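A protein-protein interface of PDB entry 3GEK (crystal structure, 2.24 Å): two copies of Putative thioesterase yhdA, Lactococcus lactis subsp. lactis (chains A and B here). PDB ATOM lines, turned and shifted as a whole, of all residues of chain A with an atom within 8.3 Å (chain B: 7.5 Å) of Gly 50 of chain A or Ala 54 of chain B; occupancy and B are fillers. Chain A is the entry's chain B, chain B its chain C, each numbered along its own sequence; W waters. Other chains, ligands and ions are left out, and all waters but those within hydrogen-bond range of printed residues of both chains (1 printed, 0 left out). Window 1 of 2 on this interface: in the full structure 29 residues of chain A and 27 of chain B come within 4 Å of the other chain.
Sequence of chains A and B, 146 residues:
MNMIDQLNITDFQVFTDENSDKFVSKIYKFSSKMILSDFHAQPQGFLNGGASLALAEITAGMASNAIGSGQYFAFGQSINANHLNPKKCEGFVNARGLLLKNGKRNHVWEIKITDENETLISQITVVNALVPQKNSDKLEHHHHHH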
ATOM      1  N   MET A   3     -24.656  16.073 -22.054  1.00  0.00           N
ATOM      2  CA  MET A   3     -25.380  15.671 -20.851  1.00  0.00           C
ATOM      3  C   MET A   3     -26.770  16.301 -20.765  1.00  0.00           C
ATOM      4  O   MET A   3     -27.739  15.616 -20.432  1.00  0.00           O
ATOM      5  CB  MET A   3     -24.575  16.012 -19.596  1.00  0.00           C
ATOM      6  CG  MET A   3     -25.148  15.438 -18.320  1.00  0.00           C
ATOM      7  SD  MET A   3     -24.163  16.097 -16.782  1.00  0.00           S
ATOM      8  CE  MET A   3     -24.934  17.880 -16.630  1.00  0.00           C
ATOM      9  N   LEU A   7     -30.117  14.059 -20.583  1.00  0.00           N
ATOM     10  CA  LEU A   7     -30.935  14.155 -19.367  1.00  0.00           C
ATOM     11  C   LEU A   7     -32.430  14.192 -19.692  1.00  0.00           C
ATOM     12  O   LEU A   7     -33.259  13.854 -18.850  1.00  0.00           O
ATOM     13  CB  LEU A   7     -30.520  15.374 -18.530  1.00  0.00           C
ATOM     14  CG  LEU A   7     -29.845  15.267 -17.146  1.00  0.00           C
ATOM     15  CD1 LEU A   7     -29.375  13.884 -16.727  1.00  0.00           C
ATOM     16  CD2 LEU A   7     -28.710  16.276 -17.015  1.00  0.00           C
ATOM     17  N   MET A  34     -38.429  15.482 -16.327  1.00  0.00           N
ATOM     18  CA  MET A  34     -37.285  14.709 -16.771  1.00  0.00           C
ATOM     19  C   MET A  34     -37.731  13.287 -17.045  1.00  0.00           C
ATOM     20  O   MET A  34     -38.255  12.604 -16.155  1.00  0.00           O
ATOM     21  CB  MET A  34     -36.142  14.727 -15.761  1.00  0.00           C
ATOM     22  CG  MET A  34     -34.951  13.923 -16.243  1.00  0.00           C
ATOM     23  SD  MET A  34     -33.309  14.246 -15.273  1.00  0.00           S
ATOM     24  CE  MET A  34     -33.777  13.384 -13.577  1.00  0.00           C
ATOM     25  N   HIS A  40     -30.185   7.502 -16.846  1.00  0.00           N
ATOM     26  CA  HIS A  40     -30.292   8.089 -15.502  1.00  0.00           C
ATOM     27  C   HIS A  40     -30.031   7.126 -14.336  1.00  0.00           C
ATOM     28  O   HIS A  40     -30.020   7.558 -13.186  1.00  0.00           O
ATOM     29  CB  HIS A  40     -31.683   8.716 -15.305  1.00  0.00           C
ATOM     30  CG  HIS A  40     -32.128   9.587 -16.439  1.00  0.00           C
ATOM     31  ND1 HIS A  40     -32.185  10.961 -16.343  1.00  0.00           N
ATOM     32  CD2 HIS A  40     -32.546   9.278 -17.690  1.00  0.00           C
ATOM     33  CE1 HIS A  40     -32.613  11.460 -17.489  1.00  0.00           C
ATOM     34  NE2 HIS A  40     -32.840  10.462 -18.322  1.00  0.00           N
ATOM     35  N   GLN A  42     -28.582   4.497 -11.510  1.00  0.00           N
ATOM     36  CA  GLN A  42     -27.450   4.047 -10.691  1.00  0.00           C
ATOM     37  C   GLN A  42     -27.505   2.512 -10.543  1.00  0.00           C
ATOM     38  O   GLN A  42     -28.515   1.900 -10.907  1.00  0.00           O
ATOM     39  CB  GLN A  42     -27.381   4.798  -9.345  1.00  0.00           C
ATOM     40  CG  GLN A  42     -28.613   4.709  -8.461  1.00  0.00           C
ATOM     41  CD  GLN A  42     -28.663   3.432  -7.642  1.00  0.00           C
ATOM     42  OE1 GLN A  42     -29.448   2.533  -7.933  1.00  0.00           O
ATOM     43  NE2 GLN A  42     -27.819   3.345  -6.614  1.00  0.00           N
ATOM     44  N   LEU A  47     -33.103   5.955  -9.641  1.00  0.00           N
ATOM     45  CA  LEU A  47     -32.685   7.206 -10.250  1.00  0.00           C
ATOM     46  C   LEU A  47     -31.443   7.698  -9.516  1.00  0.00           C
ATOM     47  O   LEU A  47     -31.457   7.873  -8.294  1.00  0.00           O
ATOM     48  CB  LEU A  47     -33.800   8.255 -10.188  1.00  0.00           C
ATOM     49  CG  LEU A  47     -33.446   9.710 -10.541  1.00  0.00           C
ATOM     50  CD1 LEU A  47     -32.877   9.853 -11.963  1.00  0.00           C
ATOM     51  CD2 LEU A  47     -34.661  10.613 -10.348  1.00  0.00           C
ATOM     52  N   ASN A  48     -30.370   7.881 -10.281  1.00  0.00           N
ATOM     53  CA  ASN A  48     -29.111   8.426  -9.795  1.00  0.00           C
ATOM     54  C   ASN A  48     -29.308   9.835  -9.253  1.00  0.00           C
ATOM     55  O   ASN A  48     -29.727  10.734  -9.990  1.00  0.00           O
ATOM     56  CB  ASN A  48     -28.105   8.445 -10.945  1.00  0.00           C
ATOM     57  CG  ASN A  48     -26.696   8.776 -10.501  1.00  0.00           C
ATOM     58  OD1 ASN A  48     -26.473   9.512  -9.537  1.00  0.00           O
ATOM     59  ND2 ASN A  48     -25.728   8.242 -11.226  1.00  0.00           N
ATOM     60  N   GLY A  49     -29.004  10.024  -7.969  1.00  0.00           N
ATOM     61  CA  GLY A  49     -29.123  11.331  -7.314  1.00  0.00           C
ATOM     62  C   GLY A  49     -28.362  12.418  -8.048  1.00  0.00           C
ATOM     63  O   GLY A  49     -28.771  13.585  -8.046  1.00  0.00           O
ATOM     64  N   GLY A  50     -27.258  12.025  -8.682  1.00  0.00           N
ATOM     65  CA  GLY A  50     -26.448  12.915  -9.501  1.00  0.00           C
ATOM     66  C   GLY A  50     -27.200  13.444 -10.704  1.00  0.00           C
ATOM     67  O   GLY A  50     -26.943  14.562 -11.154  1.00  0.00           O
ATOM     68  N   ALA A  51     -28.126  12.644 -11.232  1.00  0.00           N
ATOM     69  CA  ALA A  51     -28.978  13.093 -12.334  1.00  0.00           C
ATOM     70  C   ALA A  51     -29.953  14.178 -11.870  1.00  0.00           C
ATOM     71  O   ALA A  51     -30.217  15.137 -12.602  1.00  0.00           O
ATOM     72  CB  ALA A  51     -29.720  11.923 -12.966  1.00  0.00           C
ATOM     73  N   SER A  52     -30.465  14.024 -10.648  1.00  0.00           N
ATOM     74  CA  SER A  52     -31.379  14.992 -10.047  1.00  0.00           C
ATOM     75  C   SER A  52     -30.680  16.295  -9.690  1.00  0.00           C
ATOM     76  O   SER A  52     -31.205  17.373  -9.970  1.00  0.00           O
ATOM     77  CB  SER A  52     -32.065  14.398  -8.816  1.00  0.00           C
ATOM     78  OG  SER A  52     -32.927  13.355  -9.216  1.00  0.00           O
ATOM     79  N   LEU A  53     -29.499  16.197  -9.080  1.00  0.00           N
ATOM     80  CA  LEU A  53     -28.639  17.368  -8.875  1.00  0.00           C
ATOM     81  C   LEU A  53     -28.474  18.155 -10.175  1.00  0.00           C
ATOM     82  O   LEU A  53     -28.721  19.366 -10.211  1.00  0.00           O
ATOM     83  CB  LEU A  53     -27.257  16.961  -8.344  1.00  0.00           C
ATOM     84  CG  LEU A  53     -27.169  16.309  -6.964  1.00  0.00           C
ATOM     85  CD1 LEU A  53     -25.737  15.954  -6.617  1.00  0.00           C
ATOM     86  CD2 LEU A  53     -27.751  17.223  -5.917  1.00  0.00           C
ATOM     87  N   ALA A  54     -28.054  17.456 -11.229  1.00  0.00           N
ATOM     88  CA  ALA A  54     -27.834  18.053 -12.543  1.00  0.00           C
ATOM     89  C   ALA A  54     -29.100  18.714 -13.063  1.00  0.00           C
ATOM     90  O   ALA A  54     -29.070  19.879 -13.462  1.00  0.00           O
ATOM     91  CB  ALA A  54     -27.340  17.001 -13.524  1.00  0.00           C
ATOM     92  N   LEU A  55     -30.208  17.970 -13.032  1.00  0.00           N
ATOM     93  CA  LEU A  55     -31.523  18.492 -13.393  1.00  0.00           C
ATOM     94  C   LEU A  55     -31.818  19.830 -12.710  1.00  0.00           C
ATOM     95  O   LEU A  55     -32.277  20.771 -13.365  1.00  0.00           O
ATOM     96  CB  LEU A  55     -32.622  17.469 -13.065  1.00  0.00           C
ATOM     97  CG  LEU A  55     -34.093  17.894 -13.217  1.00  0.00           C
ATOM     98  CD1 LEU A  55     -34.447  18.152 -14.684  1.00  0.00           C
ATOM     99  CD2 LEU A  55     -35.045  16.864 -12.617  1.00  0.00           C
ATOM    100  N   ALA A  56     -31.553  19.909 -11.403  1.00  0.00           N
ATOM    101  CA  ALA A  56     -31.824  21.124 -10.631  1.00  0.00           C
ATOM    102  C   ALA A  56     -30.947  22.299 -11.056  1.00  0.00           C
ATOM    103  O   ALA A  56     -31.458  23.395 -11.263  1.00  0.00           O
ATOM    104  CB  ALA A  56     -31.696  20.873  -9.132  1.00  0.00           C
ATOM    105  N   GLU A  57     -29.640  22.076 -11.191  1.00  0.00           N
ATOM    106  CA  GLU A  57     -28.741  23.160 -11.612  1.00  0.00           C
ATOM    107  C   GLU A  57     -29.079  23.663 -13.024  1.00  0.00           C
ATOM    108  O   GLU A  57     -29.177  24.875 -13.250  1.00  0.00           O
ATOM    109  CB  GLU A  57     -27.253  22.783 -11.488  1.00  0.00           C
ATOM    110  CG  GLU A  57     -26.321  23.889 -12.044  1.00  0.00           C
ATOM    111  CD  GLU A  57     -24.879  23.835 -11.550  1.00  0.00           C
ATOM    112  OE1 GLU A  57     -24.556  22.996 -10.679  1.00  0.00           O
ATOM    113  OE2 GLU A  57     -24.055  24.650 -12.050  1.00  0.00           O
ATOM    114  N   ILE A  58     -29.261  22.730 -13.957  1.00  0.00           N
ATOM    115  CA  ILE A  58     -29.590  23.071 -15.347  1.00  0.00           C
ATOM    116  C   ILE A  58     -30.916  23.834 -15.489  1.00  0.00           C
ATOM    117  O   ILE A  58     -30.946  24.873 -16.143  1.00  0.00           O
ATOM    118  CB  ILE A  58     -29.561  21.826 -16.275  1.00  0.00           C
ATOM    119  CG1 ILE A  58     -28.138  21.257 -16.358  1.00  0.00           C
ATOM    120  CG2 ILE A  58     -30.066  22.168 -17.685  1.00  0.00           C
ATOM    121  CD1 ILE A  58     -28.083  19.763 -16.640  1.00  0.00           C
ATOM    122  N   HIS A  83     -31.800  14.550  -0.760  1.00  0.00           N
ATOM    123  CA  HIS A  83     -32.499  13.427  -1.372  1.00  0.00           C
ATOM    124  C   HIS A  83     -33.353  12.798  -0.294  1.00  0.00           C
ATOM    125  O   HIS A  83     -32.840  12.336   0.728  1.00  0.00           O
ATOM    126  CB  HIS A  83     -31.531  12.409  -1.991  1.00  0.00           C
ATOM    127  CG  HIS A  83     -30.695  12.969  -3.104  1.00  0.00           C
ATOM    128  ND1 HIS A  83     -31.230  13.714  -4.136  1.00  0.00           N
ATOM    129  CD2 HIS A  83     -29.364  12.895  -3.344  1.00  0.00           C
ATOM    130  CE1 HIS A  83     -30.263  14.081  -4.960  1.00  0.00           C
ATOM    131  NE2 HIS A  83     -29.122  13.594  -4.504  1.00  0.00           N
ATOM    132  N   SER A 122     -36.574  14.776  -4.114  1.00  0.00           N
ATOM    133  CA  SER A 122     -35.445  15.600  -3.701  1.00  0.00           C
ATOM    134  C   SER A 122     -35.872  17.060  -3.620  1.00  0.00           C
ATOM    135  O   SER A 122     -36.713  17.514  -4.411  1.00  0.00           O
ATOM    136  CB  SER A 122     -34.282  15.462  -4.691  1.00  0.00           C
ATOM    137  OG  SER A 122     -33.763  14.136  -4.694  1.00  0.00           O
ATOM    138  N   MET B   3     -25.216   7.688 -17.871  1.00  0.00           N
ATOM    139  CA  MET B   3     -24.595   8.927 -17.425  1.00  0.00           C
ATOM    140  C   MET B   3     -23.257   8.706 -16.719  1.00  0.00           C
ATOM    141  O   MET B   3     -22.291   9.419 -16.996  1.00  0.00           O
ATOM    142  CB  MET B   3     -25.549   9.707 -16.529  1.00  0.00           C
ATOM    143  CG  MET B   3     -25.087  11.110 -16.209  1.00  0.00           C
ATOM    144  SD  MET B   3     -26.190  11.860 -14.811  1.00  0.00           S
ATOM    145  CE  MET B   3     -25.968  10.495 -13.442  1.00  0.00           C
ATOM    146  N   ILE B   4     -23.204   7.731 -15.832  1.00  0.00           N
ATOM    147  CA  ILE B   4     -21.980   7.422 -15.083  1.00  0.00           C
ATOM    148  C   ILE B   4     -20.787   7.160 -16.018  1.00  0.00           C
ATOM    149  O   ILE B   4     -19.707   7.728 -15.824  1.00  0.00           O
ATOM    150  CB  ILE B   4     -22.186   6.233 -14.103  1.00  0.00           C
ATOM    151  CG1 ILE B   4     -23.333   6.532 -13.124  1.00  0.00           C
ATOM    152  CG2 ILE B   4     -20.887   5.908 -13.345  1.00  0.00           C
ATOM    153  CD1 ILE B   4     -23.898   5.302 -12.420  1.00  0.00           C
ATOM    154  N   LEU B   7     -19.762  10.262 -18.188  1.00  0.00           N
ATOM    155  CA  LEU B   7     -19.024  11.212 -17.350  1.00  0.00           C
ATOM    156  C   LEU B   7     -17.519  10.964 -17.430  1.00  0.00           C
ATOM    157  O   LEU B   7     -16.725  11.868 -17.188  1.00  0.00           O
ATOM    158  CB  LEU B   7     -19.497  11.125 -15.893  1.00  0.00           C
ATOM    159  CG  LEU B   7     -20.401  12.175 -15.218  1.00  0.00           C
ATOM    160  CD1 LEU B   7     -21.028  13.210 -16.153  1.00  0.00           C
ATOM    161  CD2 LEU B   7     -21.469  11.488 -14.370  1.00  0.00           C
ATOM    162  N   ILE B   9     -15.222   8.943 -15.615  1.00  0.00           N
ATOM    163  CA  ILE B   9     -14.466   9.014 -14.372  1.00  0.00           C
ATOM    164  C   ILE B   9     -13.349   7.969 -14.424  1.00  0.00           C
ATOM    165  O   ILE B   9     -13.609   6.775 -14.617  1.00  0.00           O
ATOM    166  CB  ILE B   9     -15.393   8.798 -13.136  1.00  0.00           C
ATOM    167  CG1 ILE B   9     -16.569   9.786 -13.171  1.00  0.00           C
ATOM    168  CG2 ILE B   9     -14.608   8.920 -11.830  1.00  0.00           C
ATOM    169  CD1 ILE B   9     -17.700   9.479 -12.199  1.00  0.00           C
ATOM    170  N   MET B  34     -11.879  13.206 -13.799  1.00  0.00           N
ATOM    171  CA  MET B  34     -12.933  13.228 -14.801  1.00  0.00           C
ATOM    172  C   MET B  34     -12.403  13.931 -16.045  1.00  0.00           C
ATOM    173  O   MET B  34     -12.060  15.111 -15.994  1.00  0.00           O
ATOM    174  CB  MET B  34     -14.197  13.926 -14.271  1.00  0.00           C
ATOM    175  CG  MET B  34     -15.288  14.069 -15.323  1.00  0.00           C
ATOM    176  SD  MET B  34     -17.059  14.527 -14.665  1.00  0.00           S
ATOM    177  CE  MET B  34     -16.761  16.417 -14.266  1.00  0.00           C
ATOM    178  N   ASN B  48     -20.147  22.135 -17.107  1.00  0.00           N
ATOM    179  CA  ASN B  48     -21.460  22.145 -16.478  1.00  0.00           C
ATOM    180  C   ASN B  48     -21.324  21.804 -14.999  1.00  0.00           C
ATOM    181  O   ASN B  48     -20.814  20.739 -14.648  1.00  0.00           O
ATOM    182  CB  ASN B  48     -22.369  21.124 -17.170  1.00  0.00           C
ATOM    183  CG  ASN B  48     -23.846  21.358 -16.899  1.00  0.00           C
ATOM    184  OD1 ASN B  48     -24.261  21.655 -15.781  1.00  0.00           O
ATOM    185  ND2 ASN B  48     -24.651  21.203 -17.932  1.00  0.00           N
ATOM    186  N   GLY B  49     -21.777  22.712 -14.138  1.00  0.00           N
ATOM    187  CA  GLY B  49     -21.804  22.470 -12.695  1.00  0.00           C
ATOM    188  C   GLY B  49     -22.500  21.174 -12.317  1.00  0.00           C
ATOM    189  O   GLY B  49     -22.100  20.507 -11.357  1.00  0.00           O
ATOM    190  N   GLY B  50     -23.529  20.811 -13.082  1.00  0.00           N
ATOM    191  CA  GLY B  50     -24.263  19.561 -12.887  1.00  0.00           C
ATOM    192  C   GLY B  50     -23.415  18.310 -13.057  1.00  0.00           C
ATOM    193  O   GLY B  50     -23.659  17.296 -12.401  1.00  0.00           O
ATOM    194  N   ALA B  51     -22.429  18.372 -13.950  1.00  0.00           N
ATOM    195  CA  ALA B  51     -21.476  17.279 -14.124  1.00  0.00           C
ATOM    196  C   ALA B  51     -20.589  17.115 -12.883  1.00  0.00           C
ATOM    197  O   ALA B  51     -20.273  15.993 -12.481  1.00  0.00           O
ATOM    198  CB  ALA B  51     -20.620  17.505 -15.381  1.00  0.00           C
ATOM    199  N   SER B  52     -20.193  18.241 -12.288  1.00  0.00           N
ATOM    200  CA  SER B  52     -19.356  18.243 -11.089  1.00  0.00           C
ATOM    201  C   SER B  52     -20.125  17.733  -9.882  1.00  0.00           C
ATOM    202  O   SER B  52     -19.582  16.992  -9.062  1.00  0.00           O
ATOM    203  CB  SER B  52     -18.808  19.636 -10.809  1.00  0.00           C
ATOM    204  OG  SER B  52     -17.973  20.063 -11.869  1.00  0.00           O
ATOM    205  N   LEU B  53     -21.391  18.131  -9.784  1.00  0.00           N
ATOM    206  CA  LEU B  53     -22.290  17.640  -8.743  1.00  0.00           C
ATOM    207  C   LEU B  53     -22.382  16.122  -8.817  1.00  0.00           C
ATOM    208  O   LEU B  53     -22.193  15.433  -7.809  1.00  0.00           O
ATOM    209  CB  LEU B  53     -23.680  18.279  -8.891  1.00  0.00           C
ATOM    210  CG  LEU B  53     -24.024  19.544  -8.084  1.00  0.00           C
ATOM    211  CD1 LEU B  53     -22.867  20.500  -7.994  1.00  0.00           C
ATOM    212  CD2 LEU B  53     -25.258  20.250  -8.658  1.00  0.00           C
ATOM    213  N   ALA B  54     -22.643  15.614 -10.024  1.00  0.00           N
ATOM    214  CA  ALA B  54     -22.786  14.176 -10.272  1.00  0.00           C
ATOM    215  C   ALA B  54     -21.484  13.439  -9.993  1.00  0.00           C
ATOM    216  O   ALA B  54     -21.494  12.390  -9.363  1.00  0.00           O
ATOM    217  CB  ALA B  54     -23.272  13.914 -11.702  1.00  0.00           C
ATOM    218  N   LEU B  55     -20.363  14.005 -10.445  1.00  0.00           N
ATOM    219  CA  LEU B  55     -19.036  13.469 -10.125  1.00  0.00           C
ATOM    220  C   LEU B  55     -18.873  13.264  -8.617  1.00  0.00           C
ATOM    221  O   LEU B  55     -18.475  12.181  -8.173  1.00  0.00           O
ATOM    222  CB  LEU B  55     -17.934  14.388 -10.660  1.00  0.00           C
ATOM    223  CG  LEU B  55     -16.466  14.070 -10.345  1.00  0.00           C
ATOM    224  CD1 LEU B  55     -16.036  12.701 -10.874  1.00  0.00           C
ATOM    225  CD2 LEU B  55     -15.565  15.162 -10.905  1.00  0.00           C
ATOM    226  N   ALA B  56     -19.206  14.296  -7.839  1.00  0.00           N
ATOM    227  CA  ALA B  56     -19.109  14.226  -6.380  1.00  0.00           C
ATOM    228  C   ALA B  56     -19.999  13.136  -5.775  1.00  0.00           C
ATOM    229  O   ALA B  56     -19.515  12.324  -4.987  1.00  0.00           O
ATOM    230  CB  ALA B  56     -19.402  15.585  -5.738  1.00  0.00           C
ATOM    231  N   GLU B  57     -21.281  13.107  -6.146  1.00  0.00           N
ATOM    232  CA  GLU B  57     -22.193  12.080  -5.619  1.00  0.00           C
ATOM    233  C   GLU B  57     -21.758  10.666  -5.992  1.00  0.00           C
ATOM    234  O   GLU B  57     -21.745   9.780  -5.133  1.00  0.00           O
ATOM    235  CB  GLU B  57     -23.659  12.325  -6.022  1.00  0.00           C
ATOM    236  CG  GLU B  57     -24.630  11.319  -5.370  1.00  0.00           C
ATOM    237  CD  GLU B  57     -26.073  11.809  -5.271  1.00  0.00           C
ATOM    238  OE1 GLU B  57     -26.327  13.002  -5.525  1.00  0.00           O
ATOM    239  OE2 GLU B  57     -26.959  10.990  -4.924  1.00  0.00           O
ATOM    240  N   ILE B  58     -21.377  10.467  -7.256  1.00  0.00           N
ATOM    241  CA  ILE B  58     -20.940   9.155  -7.737  1.00  0.00           C
ATOM    242  C   ILE B  58     -19.708   8.667  -6.977  1.00  0.00           C
ATOM    243  O   ILE B  58     -19.737   7.592  -6.375  1.00  0.00           O
ATOM    244  CB  ILE B  58     -20.633   9.140  -9.275  1.00  0.00           C
ATOM    245  CG1 ILE B  58     -21.794   9.709 -10.110  1.00  0.00           C
ATOM    246  CG2 ILE B  58     -20.245   7.733  -9.742  1.00  0.00           C
ATOM    247  CD1 ILE B  58     -23.135   9.041  -9.894  1.00  0.00           C
ATOM    248  N   THR B  59     -18.632   9.457  -7.018  1.00  0.00           N
ATOM    249  CA  THR B  59     -17.368   9.098  -6.366  1.00  0.00           C
ATOM    250  C   THR B  59     -17.525   8.893  -4.856  1.00  0.00           C
ATOM    251  O   THR B  59     -16.973   7.937  -4.308  1.00  0.00           O
ATOM    252  CB  THR B  59     -16.228  10.111  -6.659  1.00  0.00           C
ATOM    253  OG1 THR B  59     -16.678  11.446  -6.397  1.00  0.00           O
ATOM    254  CG2 THR B  59     -15.767  10.010  -8.107  1.00  0.00           C
ATOM    255  N   ALA B  60     -18.280   9.774  -4.194  1.00  0.00           N
ATOM    256  CA  ALA B  60     -18.587   9.593  -2.770  1.00  0.00           C
ATOM    257  C   ALA B  60     -19.280   8.251  -2.514  1.00  0.00           C
ATOM    258  O   ALA B  60     -18.962   7.560  -1.548  1.00  0.00           O
ATOM    259  CB  ALA B  60     -19.433  10.734  -2.244  1.00  0.00           C
ATOM    260  N   ILE B  79     -26.302  16.913  -0.262  1.00  0.00           N
ATOM    261  CA  ILE B  79     -25.119  17.378  -0.968  1.00  0.00           C
ATOM    262  C   ILE B  79     -25.123  18.896  -0.948  1.00  0.00           C
ATOM    263  O   ILE B  79     -26.149  19.521  -1.218  1.00  0.00           O
ATOM    264  CB  ILE B  79     -25.065  16.874  -2.444  1.00  0.00           C
ATOM    265  CG1 ILE B  79     -24.935  15.347  -2.528  1.00  0.00           C
ATOM    266  CG2 ILE B  79     -23.881  17.504  -3.194  1.00  0.00           C
ATOM    267  CD1 ILE B  79     -26.260  14.578  -2.545  1.00  0.00           C
ATOM    268  N   ILE B 124     -17.400  20.480  -2.547  1.00  0.00           N
ATOM    269  CA  ILE B 124     -18.676  19.790  -2.404  1.00  0.00           C
ATOM    270  C   ILE B 124     -18.621  18.826  -1.223  1.00  0.00           C
ATOM    271  O   ILE B 124     -17.646  18.094  -1.066  1.00  0.00           O
ATOM    272  CB  ILE B 124     -19.044  19.026  -3.710  1.00  0.00           C
ATOM    273  CG1 ILE B 124     -18.955  19.967  -4.928  1.00  0.00           C
ATOM    274  CG2 ILE B 124     -20.426  18.381  -3.587  1.00  0.00           C
ATOM    275  CD1 ILE B 124     -19.170  19.317  -6.289  1.00  0.00           C
HETATM  276  O   HOH W   1     -23.780  19.090 -20.562  1.00  0.00           O
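Of the 20 printed residues of chain B, 11 touch a printed residue of chain A.
Hydrophobic or aromatic side chains of chain B that line the printed part of chain A: Met 3, Ile 4, Leu 53, Ala 54, Ile 58 and Ile 79.
Among the printed residues, 19 pairs touch across the chains.
Among the printed residues, no Asp or Glu carboxylate lies within 4 Å of a Lys or Arg side-chain nitrogen of the other chain.
The backbone carbonyl oxygen (O) of His 40 of chain A lies within hydrogen-bond range of the backbone NH (N) of Asn 48 of chain A, at 2.9 Å.
The side-chain amide oxygen (OD1) of Asn 48 of chain A lies within hydrogen-bond range of the backbone NH (N) of Gly 50 of chain A (2.8 Å).
A ring nitrogen (ND1) of His 83 of chain A sits at hydrogen-bond distance from the side-chain hydroxyl (OG) of Ser 122 of chain A, 2.6 Å away.
The side-chain amide oxygen of Asn 48 of chain B lies within hydrogen-bond range of the backbone NH of Gly 50 of chain B (2.9 Å).
Water W1 lies within hydrogen-bond range of N of Met 3 of chain A (3.5 Å) and ND2 of Asn 48 of chain B (3.5 Å).
Among the printed residues, merely in contact across the chains: Met 3 of chain A with Asn 48 of chain B (3.6 Å), Met 3 of chain A with Gly 50 of chain B (3.9 Å), Met 3 of chain A with Ala 51 of chain B (3.7 Å), Asn 48 of chain A with Met 3 of chain B (3.2 Å), Asn 48 of chain A with Ile 4 of chain B (3.5 Å), Asn 48 of chain A with Ile 58 of chain B (3.0 Å), Gly 49 of chain A with Glu 57 of chain B (3.2 Å), Gly 50 of chain A with Ala 54 of chain B (3.8 Å), Ala 51 of chain A with Met 3 of chain B (3.8 Å), Leu 53 of chain A with Leu 53 of chain B (3.8 Å), Leu 53 of chain A with Glu 57 of chain B (3.2 Å), Ala 54 of chain A with Gly 50 of chain B (3.9 Å), Glu 57 of chain A with Gly 49 of chain B (3.2 Å), Glu 57 of chain A with Leu 53 of chain B (3.5 Å), Ile 58 of chain A with Asn 48 of chain B (3.8 Å) and His 83 of chain A with Ile 79 of chain B (3.6 Å).
Met 3 of chain A touches Asn 48 of chain B, and with the chains exchanged Asn 48 of chain A touches Met 3 of chain B.
Asn 48 of chain A touches Ile 58 of chain B, and with the chains exchanged Ile 58 of chain A touches Asn 48 of chain B.
Gly 50 of chain A touches Glu 57 of chain B, and with the chains exchanged Glu 57 of chain A touches Gly 50 of chain B.
Leu 53 of chain A touches its own counterpart, Leu 53 of chain B.
Positions printed for both chains: 3, 7, 34, 48, 49, 50, 51, 52, 53, 54, 55, 56, 57 and 58.
Of the 19 pairs that touch across the chains among the printed residues, 15 have their exchanged pair printed and touching as well.
The side-chain carboxylate (OE1) of Glu 57 of chain B lies within hydrogen-bond range of the backbone NH (N) of Gly 50 of chain A.
The side-chain carboxylate (OE1) of Glu 57 of chain A lies within hydrogen-bond range of the backbone NH (N) of Gly 50 of chain B, 3.4 Å away.
A ring nitrogen (NE2) of His 83 of chain A lies within hydrogen-bond range of the side-chain carboxylate of Glu 57 of chain B, 3.0 Å away.
Printed residues of chain B within 4 Å of Gly 50 of chain A: Ala 54 (3.8 Å) and Glu 57 (3.4 Å).
Ala 54 of chain B touches one residue of chain A.
Gly 49 of chain A touches one residue of chain B.
Printed residues of chain B within 4 Å of Ala 51 of chain A: Met 3 (3.8 Å).
Of the printed residues of chain A, Leu 53 of chain B touches Leu 53 and Glu 57.
Ser 52 of chain A touches none of the printed residues of chain B.
The nearest residue of chain B that does not touch Gly 50 of chain A is Met 3 of chain B (4.2 Å).
The nearest residue of chain A that does not touch Ala 54 of chain B is Leu 53 of chain A (4.6 Å).
The nearest printed residue of chain A that does not touch Asn 48 of chain B is Glu 57 of chain A (4.8 Å).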
